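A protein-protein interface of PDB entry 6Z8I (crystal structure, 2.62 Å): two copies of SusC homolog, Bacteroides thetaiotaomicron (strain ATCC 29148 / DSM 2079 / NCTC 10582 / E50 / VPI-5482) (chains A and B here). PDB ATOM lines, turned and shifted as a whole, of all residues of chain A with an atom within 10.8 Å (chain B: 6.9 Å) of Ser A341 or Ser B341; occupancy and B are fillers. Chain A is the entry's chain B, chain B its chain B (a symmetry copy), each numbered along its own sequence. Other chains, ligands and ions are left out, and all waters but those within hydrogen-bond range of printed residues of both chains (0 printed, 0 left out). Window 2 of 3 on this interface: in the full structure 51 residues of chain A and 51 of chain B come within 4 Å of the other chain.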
ATOM      1  N   GLY A 235      24.398  -2.777  22.995  1.00  0.00           N
ATOM      2  CA  GLY A 235      23.231  -1.917  22.843  1.00  0.00           C
ATOM      3  C   GLY A 235      23.440  -0.658  22.001  1.00  0.00           C
ATOM      4  O   GLY A 235      23.007   0.431  22.387  1.00  0.00           O
ATOM      5  N   GLN A 236      24.076  -0.801  20.839  1.00  0.00           N
ATOM      6  CA  GLN A 236      24.521   0.328  20.025  1.00  0.00           C
ATOM      7  C   GLN A 236      23.898   0.257  18.631  1.00  0.00           C
ATOM      8  O   GLN A 236      23.173  -0.686  18.296  1.00  0.00           O
ATOM      9  CB  GLN A 236      26.050   0.345  19.904  1.00  0.00           C
ATOM     10  CG  GLN A 236      26.800   0.537  21.214  1.00  0.00           C
ATOM     11  CD  GLN A 236      28.297   0.317  21.051  1.00  0.00           C
ATOM     12  OE1 GLN A 236      28.821   0.324  19.930  1.00  0.00           O
ATOM     13  NE2 GLN A 236      28.994   0.123  22.169  1.00  0.00           N
ATOM     14  N   ILE A 237      24.190   1.276  17.813  1.00  0.00           N
ATOM     15  CA  ILE A 237      24.008   1.223  16.360  1.00  0.00           C
ATOM     16  C   ILE A 237      25.136   1.989  15.675  1.00  0.00           C
ATOM     17  O   ILE A 237      25.279   3.200  15.870  1.00  0.00           O
ATOM     18  CB  ILE A 237      22.648   1.776  15.908  1.00  0.00           C
ATOM     19  CG1 ILE A 237      21.518   0.852  16.357  1.00  0.00           C
ATOM     20  CG2 ILE A 237      22.607   1.921  14.391  1.00  0.00           C
ATOM     21  CD1 ILE A 237      20.268   0.932  15.508  1.00  0.00           C
ATOM     22  N   LYS A 238      25.914   1.290  14.844  1.00  0.00           N
ATOM     23  CA  LYS A 238      27.177   1.767  14.307  1.00  0.00           C
ATOM     24  C   LYS A 238      27.133   1.765  12.779  1.00  0.00           C
ATOM     25  O   LYS A 238      26.502   0.904  12.155  1.00  0.00           O
ATOM     26  CB  LYS A 238      28.348   0.893  14.805  1.00  0.00           C
ATOM     27  CG  LYS A 238      28.174   0.251  16.196  1.00  0.00           C
ATOM     28  CD  LYS A 238      27.318  -1.033  16.170  1.00  0.00           C
ATOM     29  CE  LYS A 238      27.461  -1.874  17.445  1.00  0.00           C
ATOM     30  NZ  LYS A 238      26.321  -2.832  17.634  1.00  0.00           N
ATOM     31  N   SER A 338      25.406  -1.796  11.580  1.00  0.00           N
ATOM     32  CA  SER A 338      25.266  -2.881  12.544  1.00  0.00           C
ATOM     33  C   SER A 338      24.414  -2.424  13.719  1.00  0.00           C
ATOM     34  O   SER A 338      24.402  -1.244  14.079  1.00  0.00           O
ATOM     35  CB  SER A 338      26.620  -3.368  13.061  1.00  0.00           C
ATOM     36  OG  SER A 338      27.541  -2.301  13.184  1.00  0.00           O
ATOM     37  N   ASN A 339      23.699  -3.373  14.312  1.00  0.00           N
ATOM     38  CA  ASN A 339      22.762  -3.078  15.382  1.00  0.00           C
ATOM     39  C   ASN A 339      22.953  -4.085  16.506  1.00  0.00           C
ATOM     40  O   ASN A 339      22.791  -5.292  16.292  1.00  0.00           O
ATOM     41  CB  ASN A 339      21.324  -3.104  14.871  1.00  0.00           C
ATOM     42  CG  ASN A 339      20.328  -3.362  15.976  1.00  0.00           C
ATOM     43  OD1 ASN A 339      19.942  -2.451  16.709  1.00  0.00           O
ATOM     44  ND2 ASN A 339      19.931  -4.619  16.122  1.00  0.00           N
ATOM     45  N   GLY A 340      23.284  -3.583  17.699  1.00  0.00           N
ATOM     46  CA  GLY A 340      23.480  -4.403  18.881  1.00  0.00           C
ATOM     47  C   GLY A 340      22.351  -4.260  19.881  1.00  0.00           C
ATOM     48  O   GLY A 340      22.037  -3.155  20.336  1.00  0.00           O
ATOM     49  N   SER A 341      21.719  -5.376  20.223  1.00  0.00           N
ATOM     50  CA  SER A 341      20.547  -5.344  21.077  1.00  0.00           C
ATOM     51  C   SER A 341      20.643  -6.486  22.068  1.00  0.00           C
ATOM     52  O   SER A 341      21.309  -7.493  21.817  1.00  0.00           O
ATOM     53  CB  SER A 341      19.250  -5.447  20.262  1.00  0.00           C
ATOM     54  OG  SER A 341      18.245  -6.151  20.972  1.00  0.00           O
ATOM     55  N   GLU A 342      19.961  -6.311  23.201  1.00  0.00           N
ATOM     56  CA  GLU A 342      20.055  -7.276  24.290  1.00  0.00           C
ATOM     57  C   GLU A 342      19.877  -8.700  23.772  1.00  0.00           C
ATOM     58  O   GLU A 342      20.725  -9.565  24.006  1.00  0.00           O
ATOM     59  CB  GLU A 342      19.024  -6.941  25.379  1.00  0.00           C
ATOM     60  CG  GLU A 342      18.909  -7.965  26.510  1.00  0.00           C
ATOM     61  CD  GLU A 342      18.570  -7.328  27.863  1.00  0.00           C
ATOM     62  OE1 GLU A 342      18.646  -6.087  27.978  1.00  0.00           O
ATOM     63  OE2 GLU A 342      18.225  -8.073  28.812  1.00  0.00           O
ATOM     64  N   LYS A 343      18.830  -8.933  22.983  1.00  0.00           N
ATOM     65  CA  LYS A 343      18.422 -10.282  22.619  1.00  0.00           C
ATOM     66  C   LYS A 343      18.823 -10.681  21.204  1.00  0.00           C
ATOM     67  O   LYS A 343      18.370 -11.721  20.721  1.00  0.00           O
ATOM     68  CB  LYS A 343      16.908 -10.429  22.789  1.00  0.00           C
ATOM     69  CG  LYS A 343      16.475 -10.493  24.231  1.00  0.00           C
ATOM     70  CD  LYS A 343      15.435 -11.567  24.485  1.00  0.00           C
ATOM     71  CE  LYS A 343      15.188 -11.743  25.999  1.00  0.00           C
ATOM     72  NZ  LYS A 343      16.138 -11.018  26.918  1.00  0.00           N
ATOM     73  N   GLY A 344      19.668  -9.905  20.535  1.00  0.00           N
ATOM     74  CA  GLY A 344      20.132 -10.289  19.215  1.00  0.00           C
ATOM     75  C   GLY A 344      20.903  -9.160  18.564  1.00  0.00           C
ATOM     76  O   GLY A 344      21.028  -8.060  19.118  1.00  0.00           O
ATOM     77  N   SER A 345      21.416  -9.454  17.369  1.00  0.00           N
ATOM     78  CA  SER A 345      22.216  -8.505  16.599  1.00  0.00           C
ATOM     79  C   SER A 345      21.990  -8.742  15.097  1.00  0.00           C
ATOM     80  O   SER A 345      21.550  -9.818  14.670  1.00  0.00           O
ATOM     81  CB  SER A 345      23.704  -8.643  16.984  1.00  0.00           C
ATOM     82  OG  SER A 345      24.465  -7.485  16.692  1.00  0.00           O
ATOM     83  N   SER A 346      22.300  -7.727  14.288  1.00  0.00           N
ATOM     84  CA  SER A 346      22.140  -7.847  12.845  1.00  0.00           C
ATOM     85  C   SER A 346      23.068  -6.866  12.140  1.00  0.00           C
ATOM     86  O   SER A 346      23.337  -5.777  12.645  1.00  0.00           O
ATOM     87  CB  SER A 346      20.688  -7.607  12.414  1.00  0.00           C
ATOM     88  OG  SER A 346      20.393  -6.220  12.315  1.00  0.00           O
ATOM     89  N   PHE A 347      23.542  -7.266  10.956  1.00  0.00           N
ATOM     90  CA  PHE A 347      24.543  -6.507  10.220  1.00  0.00           C
ATOM     91  C   PHE A 347      24.145  -6.461   8.746  1.00  0.00           C
ATOM     92  O   PHE A 347      23.497  -7.378   8.236  1.00  0.00           O
ATOM     93  CB  PHE A 347      25.941  -7.129  10.416  1.00  0.00           C
ATOM     94  CG  PHE A 347      26.998  -6.559   9.515  1.00  0.00           C
ATOM     95  CD1 PHE A 347      27.799  -5.524   9.945  1.00  0.00           C
ATOM     96  CD2 PHE A 347      27.190  -7.065   8.236  1.00  0.00           C
ATOM     97  CE1 PHE A 347      28.778  -5.006   9.125  1.00  0.00           C
ATOM     98  CE2 PHE A 347      28.155  -6.533   7.404  1.00  0.00           C
ATOM     99  CZ  PHE A 347      28.945  -5.492   7.854  1.00  0.00           C
ATOM    100  N   SER A 373      22.894 -12.093  10.952  1.00  0.00           N
ATOM    101  CA  SER A 373      22.134 -11.832  12.182  1.00  0.00           C
ATOM    102  C   SER A 373      22.149 -13.041  13.122  1.00  0.00           C
ATOM    103  O   SER A 373      22.405 -14.177  12.702  1.00  0.00           O
ATOM    104  CB  SER A 373      20.689 -11.450  11.868  1.00  0.00           C
ATOM    105  OG  SER A 373      20.030 -12.522  11.228  1.00  0.00           O
ATOM    106  N   ASP A 374      21.840 -12.774  14.404  1.00  0.00           N
ATOM    107  CA  ASP A 374      21.779 -13.782  15.464  1.00  0.00           C
ATOM    108  C   ASP A 374      20.597 -13.490  16.391  1.00  0.00           C
ATOM    109  O   ASP A 374      20.156 -12.346  16.519  1.00  0.00           O
ATOM    110  CB  ASP A 374      23.085 -13.835  16.284  1.00  0.00           C
ATOM    111  CG  ASP A 374      23.325 -12.562  17.091  1.00  0.00           C
ATOM    112  OD1 ASP A 374      23.025 -11.483  16.554  1.00  0.00           O
ATOM    113  OD2 ASP A 374      23.793 -12.631  18.256  1.00  0.00           O
ATOM    114  N   TYR A 375      20.083 -14.535  17.042  1.00  0.00           N
ATOM    115  CA  TYR A 375      18.877 -14.433  17.861  1.00  0.00           C
ATOM    116  C   TYR A 375      19.039 -15.267  19.118  1.00  0.00           C
ATOM    117  O   TYR A 375      19.098 -16.497  19.040  1.00  0.00           O
ATOM    118  CB  TYR A 375      17.635 -14.909  17.108  1.00  0.00           C
ATOM    119  CG  TYR A 375      17.485 -14.329  15.729  1.00  0.00           C
ATOM    120  CD1 TYR A 375      18.227 -14.828  14.662  1.00  0.00           C
ATOM    121  CD2 TYR A 375      16.577 -13.303  15.473  1.00  0.00           C
ATOM    122  CE1 TYR A 375      18.090 -14.308  13.397  1.00  0.00           C
ATOM    123  CE2 TYR A 375      16.437 -12.778  14.191  1.00  0.00           C
ATOM    124  CZ  TYR A 375      17.201 -13.292  13.163  1.00  0.00           C
ATOM    125  OH  TYR A 375      17.085 -12.797  11.896  1.00  0.00           O
ATOM    126  N   LYS A 376      19.053 -14.607  20.274  1.00  0.00           N
ATOM    127  CA  LYS A 376      19.179 -15.307  21.553  1.00  0.00           C
ATOM    128  C   LYS A 376      17.799 -15.758  22.018  1.00  0.00           C
ATOM    129  O   LYS A 376      17.073 -15.021  22.675  1.00  0.00           O
ATOM    130  CB  LYS A 376      19.867 -14.425  22.591  1.00  0.00           C
ATOM    131  CG  LYS A 376      20.998 -13.592  22.019  1.00  0.00           C
ATOM    132  CD  LYS A 376      21.772 -12.866  23.099  1.00  0.00           C
ATOM    133  CE  LYS A 376      20.877 -12.514  24.275  1.00  0.00           C
ATOM    134  NZ  LYS A 376      21.616 -11.759  25.323  1.00  0.00           N
ATOM    135  N   LEU A 377      17.428 -16.981  21.652  1.00  0.00           N
ATOM    136  CA  LEU A 377      16.336 -17.664  22.323  1.00  0.00           C
ATOM    137  C   LEU A 377      16.814 -18.171  23.686  1.00  0.00           C
ATOM    138  O   LEU A 377      18.007 -18.118  24.002  1.00  0.00           O
ATOM    139  CB  LEU A 377      15.839 -18.827  21.469  1.00  0.00           C
ATOM    140  CG  LEU A 377      15.877 -18.635  19.948  1.00  0.00           C
ATOM    141  CD1 LEU A 377      15.171 -19.771  19.187  1.00  0.00           C
ATOM    142  CD2 LEU A 377      15.285 -17.287  19.554  1.00  0.00           C
ATOM    143  N   ASP A 379      17.203 -17.352  26.742  1.00  0.00           N
ATOM    144  CA  ASP A 379      18.315 -16.410  26.813  1.00  0.00           C
ATOM    145  C   ASP A 379      19.587 -16.988  27.414  1.00  0.00           C
ATOM    146  O   ASP A 379      19.728 -17.093  28.637  1.00  0.00           O
ATOM    147  CB  ASP A 379      17.891 -15.152  27.576  1.00  0.00           C
ATOM    148  CG  ASP A 379      16.488 -14.707  27.226  1.00  0.00           C
ATOM    149  OD1 ASP A 379      16.116 -14.822  26.039  1.00  0.00           O
ATOM    150  OD2 ASP A 379      15.756 -14.243  28.125  1.00  0.00           O
ATOM    151  N   ASP A 380      20.481 -17.415  26.519  1.00  0.00           N
ATOM    152  CA  ASP A 380      21.870 -17.787  26.775  1.00  0.00           C
ATOM    153  C   ASP A 380      22.042 -19.277  27.048  1.00  0.00           C
ATOM    154  O   ASP A 380      23.018 -19.690  27.684  1.00  0.00           O
ATOM    155  CB  ASP A 380      22.471 -16.950  27.910  1.00  0.00           C
ATOM    156  CG  ASP A 380      22.464 -15.458  27.593  1.00  0.00           C
ATOM    157  OD1 ASP A 380      23.435 -14.991  26.953  1.00  0.00           O
ATOM    158  OD2 ASP A 380      21.509 -14.749  28.006  1.00  0.00           O
ATOM    159  N   THR A 383      20.834 -20.556  20.912  1.00  0.00           N
ATOM    160  CA  THR A 383      21.094 -19.416  20.043  1.00  0.00           C
ATOM    161  C   THR A 383      21.027 -19.841  18.575  1.00  0.00           C
ATOM    162  O   THR A 383      21.544 -20.904  18.209  1.00  0.00           O
ATOM    163  CB  THR A 383      22.472 -18.800  20.380  1.00  0.00           C
ATOM    164  OG1 THR A 383      22.650 -18.787  21.802  1.00  0.00           O
ATOM    165  CG2 THR A 383      22.569 -17.380  19.883  1.00  0.00           C
ATOM    166  N   GLY B 235       9.821  -4.997  21.643  1.00  0.00           N
ATOM    167  CA  GLY B 235      10.879  -5.559  22.474  1.00  0.00           C
ATOM    168  C   GLY B 235      10.754  -7.049  22.791  1.00  0.00           C
ATOM    169  O   GLY B 235      10.943  -7.462  23.937  1.00  0.00           O
ATOM    170  N   GLN B 236      10.466  -7.865  21.777  1.00  0.00           N
ATOM    171  CA  GLN B 236      10.123  -9.274  21.956  1.00  0.00           C
ATOM    172  C   GLN B 236      11.094 -10.161  21.176  1.00  0.00           C
ATOM    173  O   GLN B 236      11.985  -9.676  20.471  1.00  0.00           O
ATOM    174  CB  GLN B 236       8.688  -9.549  21.490  1.00  0.00           C
ATOM    175  CG  GLN B 236       7.603  -8.820  22.270  1.00  0.00           C
ATOM    176  CD  GLN B 236       6.237  -8.961  21.615  1.00  0.00           C
ATOM    177  OE1 GLN B 236       6.028  -9.836  20.765  1.00  0.00           O
ATOM    178  NE2 GLN B 236       5.299  -8.101  22.007  1.00  0.00           N
ATOM    179  N   LYS B 238      10.034 -13.835  18.972  1.00  0.00           N
ATOM    180  CA  LYS B 238       8.911 -14.694  18.642  1.00  0.00           C
ATOM    181  C   LYS B 238       9.353 -15.791  17.675  1.00  0.00           C
ATOM    182  O   LYS B 238      10.220 -15.583  16.819  1.00  0.00           O
ATOM    183  CB  LYS B 238       7.759 -13.873  18.023  1.00  0.00           C
ATOM    184  CG  LYS B 238       7.635 -12.411  18.494  1.00  0.00           C
ATOM    185  CD  LYS B 238       8.611 -11.455  17.773  1.00  0.00           C
ATOM    186  CE  LYS B 238       8.236  -9.977  17.943  1.00  0.00           C
ATOM    187  NZ  LYS B 238       9.390  -9.057  17.671  1.00  0.00           N
ATOM    188  N   ASN B 339      12.835 -10.786  15.843  1.00  0.00           N
ATOM    189  CA  ASN B 339      13.418 -10.105  16.986  1.00  0.00           C
ATOM    190  C   ASN B 339      13.057  -8.629  16.927  1.00  0.00           C
ATOM    191  O   ASN B 339      13.408  -7.942  15.960  1.00  0.00           O
ATOM    192  CB  ASN B 339      14.933 -10.291  17.017  1.00  0.00           C
ATOM    193  CG  ASN B 339      15.627  -9.201  17.798  1.00  0.00           C
ATOM    194  OD1 ASN B 339      15.700  -9.247  19.027  1.00  0.00           O
ATOM    195  ND2 ASN B 339      16.115  -8.193  17.087  1.00  0.00           N
ATOM    196  N   GLY B 340      12.370  -8.147  17.966  1.00  0.00           N
ATOM    197  CA  GLY B 340      11.966  -6.756  18.079  1.00  0.00           C
ATOM    198  C   GLY B 340      12.770  -6.001  19.116  1.00  0.00           C
ATOM    199  O   GLY B 340      12.823  -6.389  20.289  1.00  0.00           O
ATOM    200  N   SER B 341      13.414  -4.921  18.695  1.00  0.00           N
ATOM    201  CA  SER B 341      14.310  -4.189  19.571  1.00  0.00           C
ATOM    202  C   SER B 341      14.090  -2.706  19.354  1.00  0.00           C
ATOM    203  O   SER B 341      13.634  -2.278  18.292  1.00  0.00           O
ATOM    204  CB  SER B 341      15.778  -4.558  19.315  1.00  0.00           C
ATOM    205  OG  SER B 341      16.637  -3.449  19.524  1.00  0.00           O
ATOM    206  N   GLU B 342      14.426  -1.927  20.384  1.00  0.00           N
ATOM    207  CA  GLU B 342      14.162  -0.493  20.358  1.00  0.00           C
ATOM    208  C   GLU B 342      14.633   0.122  19.045  1.00  0.00           C
ATOM    209  O   GLU B 342      13.859   0.784  18.347  1.00  0.00           O
ATOM    210  CB  GLU B 342      14.826   0.184  21.567  1.00  0.00           C
ATOM    211  CG  GLU B 342      14.758   1.712  21.581  1.00  0.00           C
ATOM    212  CD  GLU B 342      14.655   2.295  22.995  1.00  0.00           C
ATOM    213  OE1 GLU B 342      14.409   1.524  23.946  1.00  0.00           O
ATOM    214  OE2 GLU B 342      14.823   3.528  23.154  1.00  0.00           O
ATOM    215  N   LYS B 343      15.870  -0.168  18.646  1.00  0.00           N
ATOM    216  CA  LYS B 343      16.512   0.536  17.546  1.00  0.00           C
ATOM    217  C   LYS B 343      16.545  -0.261  16.247  1.00  0.00           C
ATOM    218  O   LYS B 343      17.226   0.151  15.305  1.00  0.00           O
ATOM    219  CB  LYS B 343      17.936   0.934  17.945  1.00  0.00           C
ATOM    220  CG  LYS B 343      17.979   2.069  18.935  1.00  0.00           C
ATOM    221  CD  LYS B 343      19.033   3.105  18.593  1.00  0.00           C
ATOM    222  CE  LYS B 343      18.894   4.348  19.499  1.00  0.00           C
ATOM    223  NZ  LYS B 343      17.658   4.408  20.362  1.00  0.00           N
ATOM    224  N   GLY B 344      15.821  -1.371  16.158  1.00  0.00           N
ATOM    225  CA  GLY B 344      15.767  -2.118  14.915  1.00  0.00           C
ATOM    226  C   GLY B 344      15.069  -3.446  15.113  1.00  0.00           C
ATOM    227  O   GLY B 344      14.676  -3.810  16.229  1.00  0.00           O
ATOM    228  N   SER B 345      14.924  -4.169  14.001  1.00  0.00           N
ATOM    229  CA  SER B 345      14.250  -5.464  13.985  1.00  0.00           C
ATOM    230  C   SER B 345      14.887  -6.362  12.912  1.00  0.00           C
ATOM    231  O   SER B 345      15.545  -5.887  11.977  1.00  0.00           O
ATOM    232  CB  SER B 345      12.739  -5.264  13.742  1.00  0.00           C
ATOM    233  OG  SER B 345      11.953  -6.351  14.192  1.00  0.00           O
ATOM    234  N   SER B 346      14.685  -7.674  13.047  1.00  0.00           N
ATOM    235  CA  SER B 346      15.231  -8.616  12.080  1.00  0.00           C
ATOM    236  C   SER B 346      14.413  -9.901  12.095  1.00  0.00           C
ATOM    237  O   SER B 346      13.896 -10.310  13.135  1.00  0.00           O
ATOM    238  CB  SER B 346      16.707  -8.924  12.358  1.00  0.00           C
ATOM    239  OG  SER B 346      16.855  -9.907  13.374  1.00  0.00           O
ATOM    240  N   ASP B 374      15.678  -4.098   9.594  1.00  0.00           N
ATOM    241  CA  ASP B 374      15.575  -2.637   9.560  1.00  0.00           C
ATOM    242  C   ASP B 374      16.431  -2.030  10.674  1.00  0.00           C
ATOM    243  O   ASP B 374      16.688  -2.666  11.698  1.00  0.00           O
ATOM    244  CB  ASP B 374      14.115  -2.161   9.704  1.00  0.00           C
ATOM    245  CG  ASP B 374      13.527  -2.472  11.077  1.00  0.00           C
ATOM    246  OD1 ASP B 374      13.830  -3.561  11.593  1.00  0.00           O
ATOM    247  OD2 ASP B 374      12.781  -1.637  11.650  1.00  0.00           O
ATOM    248  N   LYS B 376      17.022   1.715  12.755  1.00  0.00           N
ATOM    249  CA  LYS B 376      16.647   3.102  13.034  1.00  0.00           C
ATOM    250  C   LYS B 376      17.899   3.904  13.367  1.00  0.00           C
ATOM    251  O   LYS B 376      18.338   3.961  14.510  1.00  0.00           O
ATOM    252  CB  LYS B 376      15.614   3.172  14.155  1.00  0.00           C
ATOM    253  CG  LYS B 376      14.584   2.060  14.095  1.00  0.00           C
ATOM    254  CD  LYS B 376      13.476   2.257  15.107  1.00  0.00           C
ATOM    255  CE  LYS B 376      13.983   2.970  16.348  1.00  0.00           C
ATOM    256  NZ  LYS B 376      12.914   3.128  17.370  1.00  0.00           N
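Ser A341 touches its own counterpart, Ser B341.
Of the 5 pairs that touch across the chains among the printed residues, 1 has its exchanged pair printed and touching as well.
Printed residues of chain B within 4 Å of Ile A237: Lys B343 and Lys B376.
Asn A339 touches none of the printed residues of chain B.
Gly A340 touches none of the printed residues of chain B.
Ser A341 touches one residue of chain B.
Of the printed residues of chain B, Tyr A375 touches Asn B339 (3.8 Å) and Ser B346 (3.0 Å).
No residue of chain A comes within 4 Å of Gly B235.
No residue of chain A comes within 4 Å of Gly B340.
Ser B341 touches just one residue of chain A: Ser A341.
Of the printed residues of chain A, Lys B343 touches Ile A237.
The nearest printed residue of chain A that does not touch Lys B343 is Asn A339 (4.01 Å).
Printed residues of chain A that touch a printed residue of chain B: Ile A237, Ser A341 and Tyr A375.
N of Lys B343 lies close to OG of Ser B341 (3.5 Å).
The backbone carbonyl oxygen (O) of Glu B342 lies within hydrogen-bond range of the side-chain amino group (NZ) of Lys B376.
The side-chain hydroxyl (OH) of Tyr A375 sits at hydrogen-bond distance from the side-chain hydroxyl (OG) of Ser A373.
The side-chain hydroxyl (OG) of Ser A341 sits close to the backbone NH (N) of Lys A343 (3.5 Å).
O of Asn B339 is in hydrogen-bond range of OG of Ser B345 (2.8 Å).
The backbone NH (N) of Asn B339 lies within hydrogen-bond range of the backbone carbonyl oxygen (O) of Ser B346 (2.9 Å).
OG of Ser B341 lies close to OG of Ser A341 (3.5 Å).
The side-chain hydroxyl of Tyr A375 lies close to the side-chain hydroxyl of Ser B346.
Among the printed residues, pairs that only touch across the chains: Ile A237 with Lys B343 (3.1 Å), Ile A237 with Lys B376 (3.7 Å) and Tyr A375 with Asn B339 (3.8 Å).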
